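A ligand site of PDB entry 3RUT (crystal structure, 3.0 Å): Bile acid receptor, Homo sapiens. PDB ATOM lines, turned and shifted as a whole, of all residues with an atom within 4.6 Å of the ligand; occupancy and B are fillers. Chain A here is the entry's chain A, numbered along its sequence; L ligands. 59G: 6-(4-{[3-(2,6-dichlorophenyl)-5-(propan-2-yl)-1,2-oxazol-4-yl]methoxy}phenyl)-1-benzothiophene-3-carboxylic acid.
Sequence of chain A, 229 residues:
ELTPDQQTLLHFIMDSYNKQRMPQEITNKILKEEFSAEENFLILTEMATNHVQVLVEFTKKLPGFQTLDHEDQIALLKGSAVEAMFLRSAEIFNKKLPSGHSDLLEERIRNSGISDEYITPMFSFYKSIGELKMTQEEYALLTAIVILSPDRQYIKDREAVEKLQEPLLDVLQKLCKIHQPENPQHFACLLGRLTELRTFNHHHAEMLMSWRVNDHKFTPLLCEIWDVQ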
ATOM      1  N   MET A  22     -25.074   6.035 -10.073  1.00  0.00           N
ATOM      2  CA  MET A  22     -24.007   5.232  -9.447  1.00  0.00           C
ATOM      3  C   MET A  22     -24.056   5.354  -7.917  1.00  0.00           C
ATOM      4  O   MET A  22     -23.761   6.414  -7.372  1.00  0.00           O
ATOM      5  CB  MET A  22     -22.614   5.677  -9.942  1.00  0.00           C
ATOM      6  CG  MET A  22     -22.329   5.349 -11.399  1.00  0.00           C
ATOM      7  SD  MET A  22     -22.033   3.596 -11.725  1.00  0.00           S
ATOM      8  CE  MET A  22     -20.478   3.327 -10.865  1.00  0.00           C
ATOM      9  N   THR A  27     -19.194   3.409  -5.447  1.00  0.00           N
ATOM     10  CA  THR A  27     -18.120   4.300  -5.895  1.00  0.00           C
ATOM     11  C   THR A  27     -17.117   4.613  -4.783  1.00  0.00           C
ATOM     12  O   THR A  27     -15.951   4.876  -5.063  1.00  0.00           O
ATOM     13  CB  THR A  27     -18.654   5.632  -6.473  1.00  0.00           C
ATOM     14  OG1 THR A  27     -19.294   6.385  -5.453  1.00  0.00           O
ATOM     15  CG2 THR A  27     -19.637   5.368  -7.614  1.00  0.00           C
ATOM     16  N   ILE A  30     -13.483   3.003  -4.568  1.00  0.00           N
ATOM     17  CA  ILE A  30     -12.313   3.601  -5.194  1.00  0.00           C
ATOM     18  C   ILE A  30     -11.371   4.167  -4.112  1.00  0.00           C
ATOM     19  O   ILE A  30     -10.156   4.078  -4.239  1.00  0.00           O
ATOM     20  CB  ILE A  30     -12.713   4.716  -6.199  1.00  0.00           C
ATOM     21  CG1 ILE A  30     -13.464   4.112  -7.393  1.00  0.00           C
ATOM     22  CG2 ILE A  30     -11.492   5.472  -6.692  1.00  0.00           C
ATOM     23  CD1 ILE A  30     -14.374   5.099  -8.101  1.00  0.00           C
ATOM     24  N   PHE A  41      -8.274  -3.947 -10.427  1.00  0.00           N
ATOM     25  CA  PHE A  41      -9.005  -4.504 -11.555  1.00  0.00           C
ATOM     26  C   PHE A  41     -10.451  -4.840 -11.197  1.00  0.00           C
ATOM     27  O   PHE A  41     -11.347  -4.628 -12.026  1.00  0.00           O
ATOM     28  CB  PHE A  41      -8.310  -5.742 -12.105  1.00  0.00           C
ATOM     29  CG  PHE A  41      -9.102  -6.424 -13.168  1.00  0.00           C
ATOM     30  CD1 PHE A  41     -10.009  -7.413 -12.830  1.00  0.00           C
ATOM     31  CD2 PHE A  41      -8.980  -6.045 -14.497  1.00  0.00           C
ATOM     32  CE1 PHE A  41     -10.775  -8.022 -13.809  1.00  0.00           C
ATOM     33  CE2 PHE A  41      -9.733  -6.658 -15.481  1.00  0.00           C
ATOM     34  CZ  PHE A  41     -10.640  -7.646 -15.143  1.00  0.00           C
ATOM     35  N   LEU A  44     -12.468  -1.535 -10.817  1.00  0.00           N
ATOM     36  CA  LEU A  44     -12.761  -0.999 -12.133  1.00  0.00           C
ATOM     37  C   LEU A  44     -13.853  -1.794 -12.840  1.00  0.00           C
ATOM     38  O   LEU A  44     -14.719  -1.219 -13.477  1.00  0.00           O
ATOM     39  CB  LEU A  44     -11.508  -0.947 -12.986  1.00  0.00           C
ATOM     40  CG  LEU A  44     -10.513   0.133 -12.565  1.00  0.00           C
ATOM     41  CD1 LEU A  44      -9.196  -0.061 -13.290  1.00  0.00           C
ATOM     42  CD2 LEU A  44     -11.106   1.496 -12.856  1.00  0.00           C
ATOM     43  N   THR A  45     -13.790  -3.123 -12.727  1.00  0.00           N
ATOM     44  CA  THR A  45     -14.822  -3.988 -13.311  1.00  0.00           C
ATOM     45  C   THR A  45     -16.179  -3.723 -12.671  1.00  0.00           C
ATOM     46  O   THR A  45     -17.202  -3.718 -13.356  1.00  0.00           O
ATOM     47  CB  THR A  45     -14.464  -5.483 -13.143  1.00  0.00           C
ATOM     48  OG1 THR A  45     -13.205  -5.761 -13.762  1.00  0.00           O
ATOM     49  CG2 THR A  45     -15.541  -6.371 -13.769  1.00  0.00           C
ATOM     50  N   MET A  47     -17.141  -0.849 -11.238  1.00  0.00           N
ATOM     51  CA  MET A  47     -17.612   0.461 -11.673  1.00  0.00           C
ATOM     52  C   MET A  47     -18.278   0.337 -13.051  1.00  0.00           C
ATOM     53  O   MET A  47     -19.408   0.779 -13.254  1.00  0.00           O
ATOM     54  CB  MET A  47     -16.455   1.461 -11.740  1.00  0.00           C
ATOM     55  CG  MET A  47     -15.733   1.746 -10.426  1.00  0.00           C
ATOM     56  SD  MET A  47     -16.809   2.198  -9.037  1.00  0.00           S
ATOM     57  CE  MET A  47     -17.018   0.616  -8.226  1.00  0.00           C
ATOM     58  N   ALA A  48     -17.555  -0.274 -13.991  1.00  0.00           N
ATOM     59  CA  ALA A  48     -18.026  -0.442 -15.373  1.00  0.00           C
ATOM     60  C   ALA A  48     -19.352  -1.195 -15.475  1.00  0.00           C
ATOM     61  O   ALA A  48     -20.224  -0.830 -16.248  1.00  0.00           O
ATOM     62  CB  ALA A  48     -16.953  -1.145 -16.181  1.00  0.00           C
ATOM     63  N   HIS A  51     -22.044   0.952 -14.376  1.00  0.00           N
ATOM     64  CA  HIS A  51     -22.224   2.059 -15.295  1.00  0.00           C
ATOM     65  C   HIS A  51     -22.965   1.610 -16.546  1.00  0.00           C
ATOM     66  O   HIS A  51     -23.762   2.375 -17.094  1.00  0.00           O
ATOM     67  CB  HIS A  51     -20.886   2.695 -15.660  1.00  0.00           C
ATOM     68  CG  HIS A  51     -21.020   4.051 -16.284  1.00  0.00           C
ATOM     69  ND1 HIS A  51     -20.587   4.329 -17.565  1.00  0.00           N
ATOM     70  CD2 HIS A  51     -21.571   5.194 -15.823  1.00  0.00           C
ATOM     71  CE1 HIS A  51     -20.845   5.587 -17.853  1.00  0.00           C
ATOM     72  NE2 HIS A  51     -21.441   6.140 -16.807  1.00  0.00           N
ATOM     73  N   VAL A  82     -18.553   1.565 -24.659  1.00  0.00           N
ATOM     74  CA  VAL A  82     -17.159   1.891 -24.379  1.00  0.00           C
ATOM     75  C   VAL A  82     -16.890   3.381 -24.494  1.00  0.00           C
ATOM     76  O   VAL A  82     -16.222   3.966 -23.648  1.00  0.00           O
ATOM     77  CB  VAL A  82     -16.186   1.135 -25.302  1.00  0.00           C
ATOM     78  CG1 VAL A  82     -14.930   1.946 -25.554  1.00  0.00           C
ATOM     79  CG2 VAL A  82     -15.840  -0.209 -24.699  1.00  0.00           C
ATOM     80  N   MET A  85     -18.325   5.295 -21.721  1.00  0.00           N
ATOM     81  CA  MET A  85     -17.537   5.119 -20.505  1.00  0.00           C
ATOM     82  C   MET A  85     -16.288   5.991 -20.483  1.00  0.00           C
ATOM     83  O   MET A  85     -15.969   6.571 -19.451  1.00  0.00           O
ATOM     84  CB  MET A  85     -17.143   3.651 -20.325  1.00  0.00           C
ATOM     85  CG  MET A  85     -18.280   2.797 -19.816  1.00  0.00           C
ATOM     86  SD  MET A  85     -17.966   1.033 -19.920  1.00  0.00           S
ATOM     87  CE  MET A  85     -19.437   0.431 -19.102  1.00  0.00           C
ATOM     88  N   PHE A  86     -15.577   6.083 -21.604  1.00  0.00           N
ATOM     89  CA  PHE A  86     -14.430   7.003 -21.722  1.00  0.00           C
ATOM     90  C   PHE A  86     -14.871   8.416 -21.396  1.00  0.00           C
ATOM     91  O   PHE A  86     -14.121   9.181 -20.784  1.00  0.00           O
ATOM     92  CB  PHE A  86     -13.849   7.006 -23.134  1.00  0.00           C
ATOM     93  CG  PHE A  86     -12.646   6.125 -23.306  1.00  0.00           C
ATOM     94  CD1 PHE A  86     -12.790   4.809 -23.731  1.00  0.00           C
ATOM     95  CD2 PHE A  86     -11.376   6.623 -23.104  1.00  0.00           C
ATOM     96  CE1 PHE A  86     -11.684   3.986 -23.919  1.00  0.00           C
ATOM     97  CE2 PHE A  86     -10.250   5.813 -23.291  1.00  0.00           C
ATOM     98  CZ  PHE A  86     -10.408   4.486 -23.702  1.00  0.00           C
ATOM     99  N   ARG A  88     -17.545   9.522 -19.528  1.00  0.00           N
ATOM    100  CA  ARG A  88     -17.916   9.723 -18.127  1.00  0.00           C
ATOM    101  C   ARG A  88     -16.682   9.766 -17.225  1.00  0.00           C
ATOM    102  O   ARG A  88     -16.606  10.603 -16.334  1.00  0.00           O
ATOM    103  CB  ARG A  88     -18.897   8.647 -17.656  1.00  0.00           C
ATOM    104  CG  ARG A  88     -19.409   8.820 -16.239  1.00  0.00           C
ATOM    105  CD  ARG A  88     -20.013  10.193 -15.994  1.00  0.00           C
ATOM    106  NE  ARG A  88     -20.614  10.282 -14.654  1.00  0.00           N
ATOM    107  CZ  ARG A  88     -21.039  11.412 -14.082  1.00  0.00           C
ATOM    108  NH1 ARG A  88     -20.935  12.580 -14.713  1.00  0.00           N
ATOM    109  NH2 ARG A  88     -21.565  11.369 -12.865  1.00  0.00           N
ATOM    110  N   SER A  89     -15.730   8.864 -17.458  1.00  0.00           N
ATOM    111  CA  SER A  89     -14.466   8.854 -16.721  1.00  0.00           C
ATOM    112  C   SER A  89     -13.644  10.117 -16.995  1.00  0.00           C
ATOM    113  O   SER A  89     -12.951  10.608 -16.110  1.00  0.00           O
ATOM    114  CB  SER A  89     -13.642   7.609 -17.063  1.00  0.00           C
ATOM    115  OG  SER A  89     -13.178   7.655 -18.400  1.00  0.00           O
ATOM    116  N   ILE A  92     -14.955  12.720 -14.912  1.00  0.00           N
ATOM    117  CA  ILE A  92     -14.452  12.496 -13.558  1.00  0.00           C
ATOM    118  C   ILE A  92     -13.098  13.160 -13.344  1.00  0.00           C
ATOM    119  O   ILE A  92     -12.912  13.888 -12.375  1.00  0.00           O
ATOM    120  CB  ILE A  92     -14.286  10.989 -13.239  1.00  0.00           C
ATOM    121  CG1 ILE A  92     -15.643  10.276 -13.166  1.00  0.00           C
ATOM    122  CG2 ILE A  92     -13.496  10.805 -11.940  1.00  0.00           C
ATOM    123  CD1 ILE A  92     -16.508  10.738 -12.037  1.00  0.00           C
ATOM    124  N   SER A  99     -17.556  12.061  -6.529  1.00  0.00           N
ATOM    125  CA  SER A  99     -17.902  10.635  -6.560  1.00  0.00           C
ATOM    126  C   SER A  99     -16.922   9.812  -7.404  1.00  0.00           C
ATOM    127  O   SER A  99     -16.939   8.581  -7.340  1.00  0.00           O
ATOM    128  CB  SER A  99     -19.326  10.439  -7.091  1.00  0.00           C
ATOM    129  OG  SER A  99     -19.411  10.669  -8.495  1.00  0.00           O
ATOM    130  N   GLY A 100     -16.113  10.488  -8.206  1.00  0.00           N
ATOM    131  CA  GLY A 100     -15.104   9.816  -9.025  1.00  0.00           C
ATOM    132  C   GLY A 100     -13.810   9.527  -8.280  1.00  0.00           C
ATOM    133  O   GLY A 100     -13.100   8.581  -8.619  1.00  0.00           O
ATOM    134  N   ILE A 109      -6.565   2.615 -12.427  1.00  0.00           N
ATOM    135  CA  ILE A 109      -6.428   2.399 -13.866  1.00  0.00           C
ATOM    136  C   ILE A 109      -4.963   2.156 -14.225  1.00  0.00           C
ATOM    137  O   ILE A 109      -4.655   1.217 -14.963  1.00  0.00           O
ATOM    138  CB  ILE A 109      -6.976   3.586 -14.683  1.00  0.00           C
ATOM    139  CG1 ILE A 109      -8.498   3.669 -14.567  1.00  0.00           C
ATOM    140  CG2 ILE A 109      -6.590   3.445 -16.138  1.00  0.00           C
ATOM    141  CD1 ILE A 109      -9.106   4.860 -15.267  1.00  0.00           C
ATOM    142  N   ILE A 114      -3.287  -3.038 -17.531  1.00  0.00           N
ATOM    143  CA  ILE A 114      -3.315  -2.331 -18.806  1.00  0.00           C
ATOM    144  C   ILE A 114      -1.894  -1.961 -19.223  1.00  0.00           C
ATOM    145  O   ILE A 114      -1.143  -1.384 -18.445  1.00  0.00           O
ATOM    146  CB  ILE A 114      -4.129  -1.019 -18.744  1.00  0.00           C
ATOM    147  CG1 ILE A 114      -5.534  -1.248 -18.171  1.00  0.00           C
ATOM    148  CG2 ILE A 114      -4.243  -0.413 -20.143  1.00  0.00           C
ATOM    149  CD1 ILE A 114      -6.315   0.023 -17.976  1.00  0.00           C
ATOM    150  N   MET A 122      -4.601   7.053 -23.583  1.00  0.00           N
ATOM    151  CA  MET A 122      -5.755   7.194 -22.716  1.00  0.00           C
ATOM    152  C   MET A 122      -5.694   8.514 -21.964  1.00  0.00           C
ATOM    153  O   MET A 122      -6.581   9.346 -22.100  1.00  0.00           O
ATOM    154  CB  MET A 122      -5.812   6.026 -21.738  1.00  0.00           C
ATOM    155  CG  MET A 122      -7.112   5.885 -20.995  1.00  0.00           C
ATOM    156  SD  MET A 122      -7.178   4.300 -20.119  1.00  0.00           S
ATOM    157  CE  MET A 122      -6.942   3.136 -21.460  1.00  0.00           C
ATOM    158  N   TYR A 126      -7.544  12.139 -22.009  1.00  0.00           N
ATOM    159  CA  TYR A 126      -8.138  12.754 -20.824  1.00  0.00           C
ATOM    160  C   TYR A 126      -7.591  14.173 -20.600  1.00  0.00           C
ATOM    161  O   TYR A 126      -8.356  15.094 -20.285  1.00  0.00           O
ATOM    162  CB  TYR A 126      -7.843  11.919 -19.566  1.00  0.00           C
ATOM    163  CG  TYR A 126      -8.651  10.646 -19.402  1.00  0.00           C
ATOM    164  CD1 TYR A 126     -10.018  10.597 -19.656  1.00  0.00           C
ATOM    165  CD2 TYR A 126      -8.037   9.486 -18.943  1.00  0.00           C
ATOM    166  CE1 TYR A 126     -10.753   9.421 -19.494  1.00  0.00           C
ATOM    167  CE2 TYR A 126      -8.757   8.300 -18.773  1.00  0.00           C
ATOM    168  CZ  TYR A 126     -10.105   8.270 -19.037  1.00  0.00           C
ATOM    169  OH  TYR A 126     -10.798   7.101 -18.849  1.00  0.00           O
ATOM    170  N   HIS A 204      -9.814  -1.011 -27.719  1.00  0.00           N
ATOM    171  CA  HIS A 204     -10.354  -1.606 -26.484  1.00  0.00           C
ATOM    172  C   HIS A 204     -10.453  -3.127 -26.505  1.00  0.00           C
ATOM    173  O   HIS A 204     -10.270  -3.782 -25.482  1.00  0.00           O
ATOM    174  CB  HIS A 204     -11.726  -0.997 -26.165  1.00  0.00           C
ATOM    175  CG  HIS A 204     -12.282  -1.421 -24.848  1.00  0.00           C
ATOM    176  ND1 HIS A 204     -13.232  -2.414 -24.725  1.00  0.00           N
ATOM    177  CD2 HIS A 204     -12.003  -1.001 -23.589  1.00  0.00           C
ATOM    178  CE1 HIS A 204     -13.518  -2.581 -23.447  1.00  0.00           C
ATOM    179  NE2 HIS A 204     -12.784  -1.740 -22.742  1.00  0.00           N
ATOM    180  N   MET A 207      -7.231  -4.675 -25.238  1.00  0.00           N
ATOM    181  CA  MET A 207      -7.172  -4.605 -23.779  1.00  0.00           C
ATOM    182  C   MET A 207      -7.864  -5.805 -23.146  1.00  0.00           C
ATOM    183  O   MET A 207      -7.288  -6.477 -22.297  1.00  0.00           O
ATOM    184  CB  MET A 207      -7.778  -3.304 -23.249  1.00  0.00           C
ATOM    185  CG  MET A 207      -6.773  -2.181 -23.016  1.00  0.00           C
ATOM    186  SD  MET A 207      -7.537  -0.578 -22.688  1.00  0.00           S
ATOM    187  CE  MET A 207      -8.387  -0.885 -21.147  1.00  0.00           C
ATOM    188  N   LEU A 208      -9.091  -6.075 -23.576  1.00  0.00           N
ATOM    189  CA  LEU A 208      -9.861  -7.193 -23.040  1.00  0.00           C
ATOM    190  C   LEU A 208      -9.188  -8.537 -23.286  1.00  0.00           C
ATOM    191  O   LEU A 208      -9.193  -9.400 -22.416  1.00  0.00           O
ATOM    192  CB  LEU A 208     -11.279  -7.219 -23.605  1.00  0.00           C
ATOM    193  CG  LEU A 208     -12.169  -5.990 -23.424  1.00  0.00           C
ATOM    194  CD1 LEU A 208     -13.600  -6.320 -23.833  1.00  0.00           C
ATOM    195  CD2 LEU A 208     -12.140  -5.464 -21.986  1.00  0.00           C
ATOM    196  N   TRP A 211      -6.376  -9.097 -20.748  1.00  0.00           N
ATOM    197  CA  TRP A 211      -6.983  -9.489 -19.493  1.00  0.00           C
ATOM    198  C   TRP A 211      -7.479 -10.940 -19.537  1.00  0.00           C
ATOM    199  O   TRP A 211      -7.144 -11.728 -18.661  1.00  0.00           O
ATOM    200  CB  TRP A 211      -8.150  -8.571 -19.153  1.00  0.00           C
ATOM    201  CG  TRP A 211      -7.758  -7.291 -18.510  1.00  0.00           C
ATOM    202  CD1 TRP A 211      -6.829  -7.120 -17.519  1.00  0.00           C
ATOM    203  CD2 TRP A 211      -8.310  -5.994 -18.761  1.00  0.00           C
ATOM    204  NE1 TRP A 211      -6.759  -5.793 -17.162  1.00  0.00           N
ATOM    205  CE2 TRP A 211      -7.666  -5.082 -17.903  1.00  0.00           C
ATOM    206  CE3 TRP A 211      -9.287  -5.521 -19.644  1.00  0.00           C
ATOM    207  CZ2 TRP A 211      -7.963  -3.735 -17.897  1.00  0.00           C
ATOM    208  CZ3 TRP A 211      -9.592  -4.169 -19.643  1.00  0.00           C
ATOM    209  CH2 TRP A 211      -8.930  -3.295 -18.766  1.00  0.00           C
ATOM    210  N   PHE A 218     -14.407 -10.164 -15.540  1.00  0.00           N
ATOM    211  CA  PHE A 218     -15.531  -9.418 -16.102  1.00  0.00           C
ATOM    212  C   PHE A 218     -16.828  -9.936 -15.486  1.00  0.00           C
ATOM    213  O   PHE A 218     -16.790 -10.730 -14.545  1.00  0.00           O
ATOM    214  CB  PHE A 218     -15.543  -9.441 -17.645  1.00  0.00           C
ATOM    215  CG  PHE A 218     -14.262  -8.950 -18.262  1.00  0.00           C
ATOM    216  CD1 PHE A 218     -13.651  -9.667 -19.284  1.00  0.00           C
ATOM    217  CD2 PHE A 218     -13.639  -7.796 -17.811  1.00  0.00           C
ATOM    218  CE1 PHE A 218     -12.460  -9.229 -19.845  1.00  0.00           C
ATOM    219  CE2 PHE A 218     -12.452  -7.359 -18.364  1.00  0.00           C
ATOM    220  CZ  PHE A 218     -11.871  -8.078 -19.380  1.00  0.00           C
ATOM    221  N   LEU A 222     -21.078  -7.146 -18.776  1.00  0.00           N
ATOM    222  CA  LEU A 222     -19.958  -6.642 -19.585  1.00  0.00           C
ATOM    223  C   LEU A 222     -19.619  -7.571 -20.751  1.00  0.00           C
ATOM    224  O   LEU A 222     -19.342  -7.114 -21.847  1.00  0.00           O
ATOM    225  CB  LEU A 222     -18.711  -6.450 -18.727  1.00  0.00           C
ATOM    226  CG  LEU A 222     -18.638  -5.207 -17.847  1.00  0.00           C
ATOM    227  CD1 LEU A 222     -17.459  -5.310 -16.890  1.00  0.00           C
ATOM    228  CD2 LEU A 222     -18.537  -3.959 -18.719  1.00  0.00           C
ATOM    229  N   TRP A 226     -19.974  -6.479 -24.703  1.00  0.00           N
ATOM    230  CA  TRP A 226     -18.687  -6.431 -25.430  1.00  0.00           C
ATOM    231  C   TRP A 226     -18.314  -7.733 -26.126  1.00  0.00           C
ATOM    232  O   TRP A 226     -17.181  -7.898 -26.572  1.00  0.00           O
ATOM    233  CB  TRP A 226     -17.553  -6.007 -24.483  1.00  0.00           C
ATOM    234  CG  TRP A 226     -17.610  -4.581 -24.039  1.00  0.00           C
ATOM    235  CD1 TRP A 226     -18.189  -3.542 -24.703  1.00  0.00           C
ATOM    236  CD2 TRP A 226     -17.034  -4.038 -22.854  1.00  0.00           C
ATOM    237  NE1 TRP A 226     -18.040  -2.382 -23.988  1.00  0.00           N
ATOM    238  CE2 TRP A 226     -17.328  -2.660 -22.843  1.00  0.00           C
ATOM    239  CE3 TRP A 226     -16.315  -4.578 -21.783  1.00  0.00           C
ATOM    240  CZ2 TRP A 226     -16.916  -1.808 -21.815  1.00  0.00           C
ATOM    241  CZ3 TRP A 226     -15.906  -3.734 -20.758  1.00  0.00           C
ATOM    242  CH2 TRP A 226     -16.212  -2.362 -20.779  1.00  0.00           C
HETATM  243  C13 59G L   1     -16.996   3.263 -15.637  1.00  0.00           C
HETATM  244  C15 59G L   1     -15.004   3.946 -14.499  1.00  0.00           C
HETATM  245  C17 59G L   1     -17.163   4.977 -13.915  1.00  0.00           C
HETATM  246  C20 59G L   1     -18.652   6.781 -12.345  1.00  0.00           C
HETATM  247  C21 59G L   1     -19.274   7.650 -11.441  1.00  0.00           C
HETATM  248  C22 59G L   1     -18.640   7.746 -10.228  1.00  0.00           C
HETATM  249  C24 59G L   1     -17.502   6.171 -11.868  1.00  0.00           C
HETATM  250  C26 59G L   1     -20.500   8.447 -11.659  1.00  0.00           C
HETATM  251  C01 59G L   1     -12.144  -2.759 -15.636  1.00  0.00           C
HETATM  252  C02 59G L   1     -12.819  -2.929 -17.001  1.00  0.00           C
HETATM  253  C03 59G L   1     -14.333  -3.366 -16.944  1.00  0.00           C
HETATM  254  C04 59G L   1     -12.535  -1.798 -18.010  1.00  0.00           C
HETATM  255  O05 59G L   1     -12.081  -2.022 -19.257  1.00  0.00           O
HETATM  256  N06 59G L   1     -11.934  -0.820 -19.905  1.00  0.00           N
HETATM  257  C07 59G L   1     -12.301   0.153 -19.069  1.00  0.00           C
HETATM  258  C08 59G L   1     -12.674  -0.423 -17.858  1.00  0.00           C
HETATM  259  C09 59G L   1     -13.173   0.327 -16.646  1.00  0.00           C
HETATM  260  O10 59G L   1     -14.167   1.302 -17.019  1.00  0.00           O
HETATM  261  C11 59G L   1     -14.879   2.236 -16.186  1.00  0.00           C
HETATM  262  C12 59G L   1     -16.246   2.361 -16.383  1.00  0.00           C
HETATM  263  C14 59G L   1     -16.385   4.060 -14.682  1.00  0.00           C
HETATM  264  C16 59G L   1     -14.258   3.036 -15.248  1.00  0.00           C
HETATM  265  C18 59G L   1     -18.314   5.585 -14.417  1.00  0.00           C
HETATM  266  C19 59G L   1     -19.052   6.492 -13.638  1.00  0.00           C
HETATM  267  S23 59G L   1     -17.266   6.725 -10.277  1.00  0.00           S
HETATM  268  C25 59G L   1     -16.762   5.280 -12.631  1.00  0.00           C
HETATM  269  O27 59G L   1     -20.788   9.364 -10.793  1.00  0.00           O
HETATM  270  O28 59G L   1     -21.260   8.263 -12.619  1.00  0.00           O
HETATM  271  C29 59G L   1     -12.257   1.499 -19.409  1.00  0.00           C
HETATM  272  C30 59G L   1     -11.164   2.280 -19.033  1.00  0.00           C
HETATM  273 CL31 59G L   1      -9.828   1.584 -18.135  1.00  0.00          CL
HETATM  274  C32 59G L   1     -11.125   3.626 -19.365  1.00  0.00           C
HETATM  275  C33 59G L   1     -12.182   4.197 -20.084  1.00  0.00           C
HETATM  276  C34 59G L   1     -13.262   3.412 -20.464  1.00  0.00           C
HETATM  277  C35 59G L   1     -13.306   2.065 -20.124  1.00  0.00           C
HETATM  278 CL36 59G L   1     -14.626   1.136 -20.585  1.00  0.00          CL
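The side-chain hydroxyl (OG) of Ser 99 lies within hydrogen-bond range of an oxygen (O27) of the ligand (3.0 Å). The guanidinium group of Arg 88 lies within salt-bridge range of an oxygen (O28) of the ligand (2.9 Å). A ring nitrogen (NE2) of His 204 sits at hydrogen-bond distance from a nitrogen (N06) of the ligand (3.1 Å).
The backbone NH (N) of His 51 lies within hydrogen-bond range of the side-chain sulfur (SD) of Met 22 (3.7 Å). OG of Ser 89 sits at hydrogen-bond distance from OH of Tyr 126 (2.5 Å). OG1 of Thr 45 sits at hydrogen-bond distance from O of Phe 41. The side-chain hydroxyl of Ser 89 sits at hydrogen-bond distance from the backbone carbonyl oxygen of Met 85, at 3.2 Å. The backbone carbonyl oxygen (O) of Phe 86 is in hydrogen-bond range of the side-chain hydroxyl (OG) of Ser 89 (3.0 Å).
CG of Met 22 touches O28 of the ligand, at 3.3 Å. CG2 of Thr 27 touches C22 of the ligand, at 3.7 Å. CD1 of Ile 30 touches S23 of the ligand (3.97 Å). Leu 44 touches the ligand. Thr 45 touches the ligand (N to C01, 3.4 Å). CB of Met 47 touches C14 of the ligand, at 3.9 Å. Ala 48 touches the ligand. CD2 of His 51 touches C18 of the ligand, 3.6 Å away. SD of Met 85 touches CL36 of the ligand, at 3.4 Å. Phe 86 touches the ligand (CD1 to C34, 3.6 Å). Ser 89 touches the ligand (OG to C33, 3.97 Å). CA of Gly 100 touches S23 of the ligand, at 3.97 Å. Ile 114 touches the ligand. Tyr 126 touches the ligand (OH to C33, 3.4 Å). CE of Met 207 touches N06 of the ligand, 3.8 Å away. Trp 211 touches the ligand (CZ3 to O05, 3.3 Å). Leu 222 touches the ligand. Trp 226 touches the ligand. Hydrophobic or aromatic side chains within 4 Å of the ligand: Met 22, Ile 30, Leu 44, Met 47, Ala 48, His 51, Met 85, Phe 86, Ile 114, His 204, Met 207, Trp 211, Leu 222 and Trp 226. 21 residues have an atom within 4 Å of the ligand: Met 22, Thr 27, Ile 30, Leu 44, Thr 45, Met 47, Ala 48, His 51, Met 85, Phe 86, Arg 88, Ser 89, Ser 99, Gly 100, Ile 114, Tyr 126, His 204, Met 207, Trp 211, Leu 222 and Trp 226. Along chain A the residues within 4 Å of the ligand span positions 22 to 226. The nearest printed residue that does not touch the ligand is Met 122 (4.1 Å).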
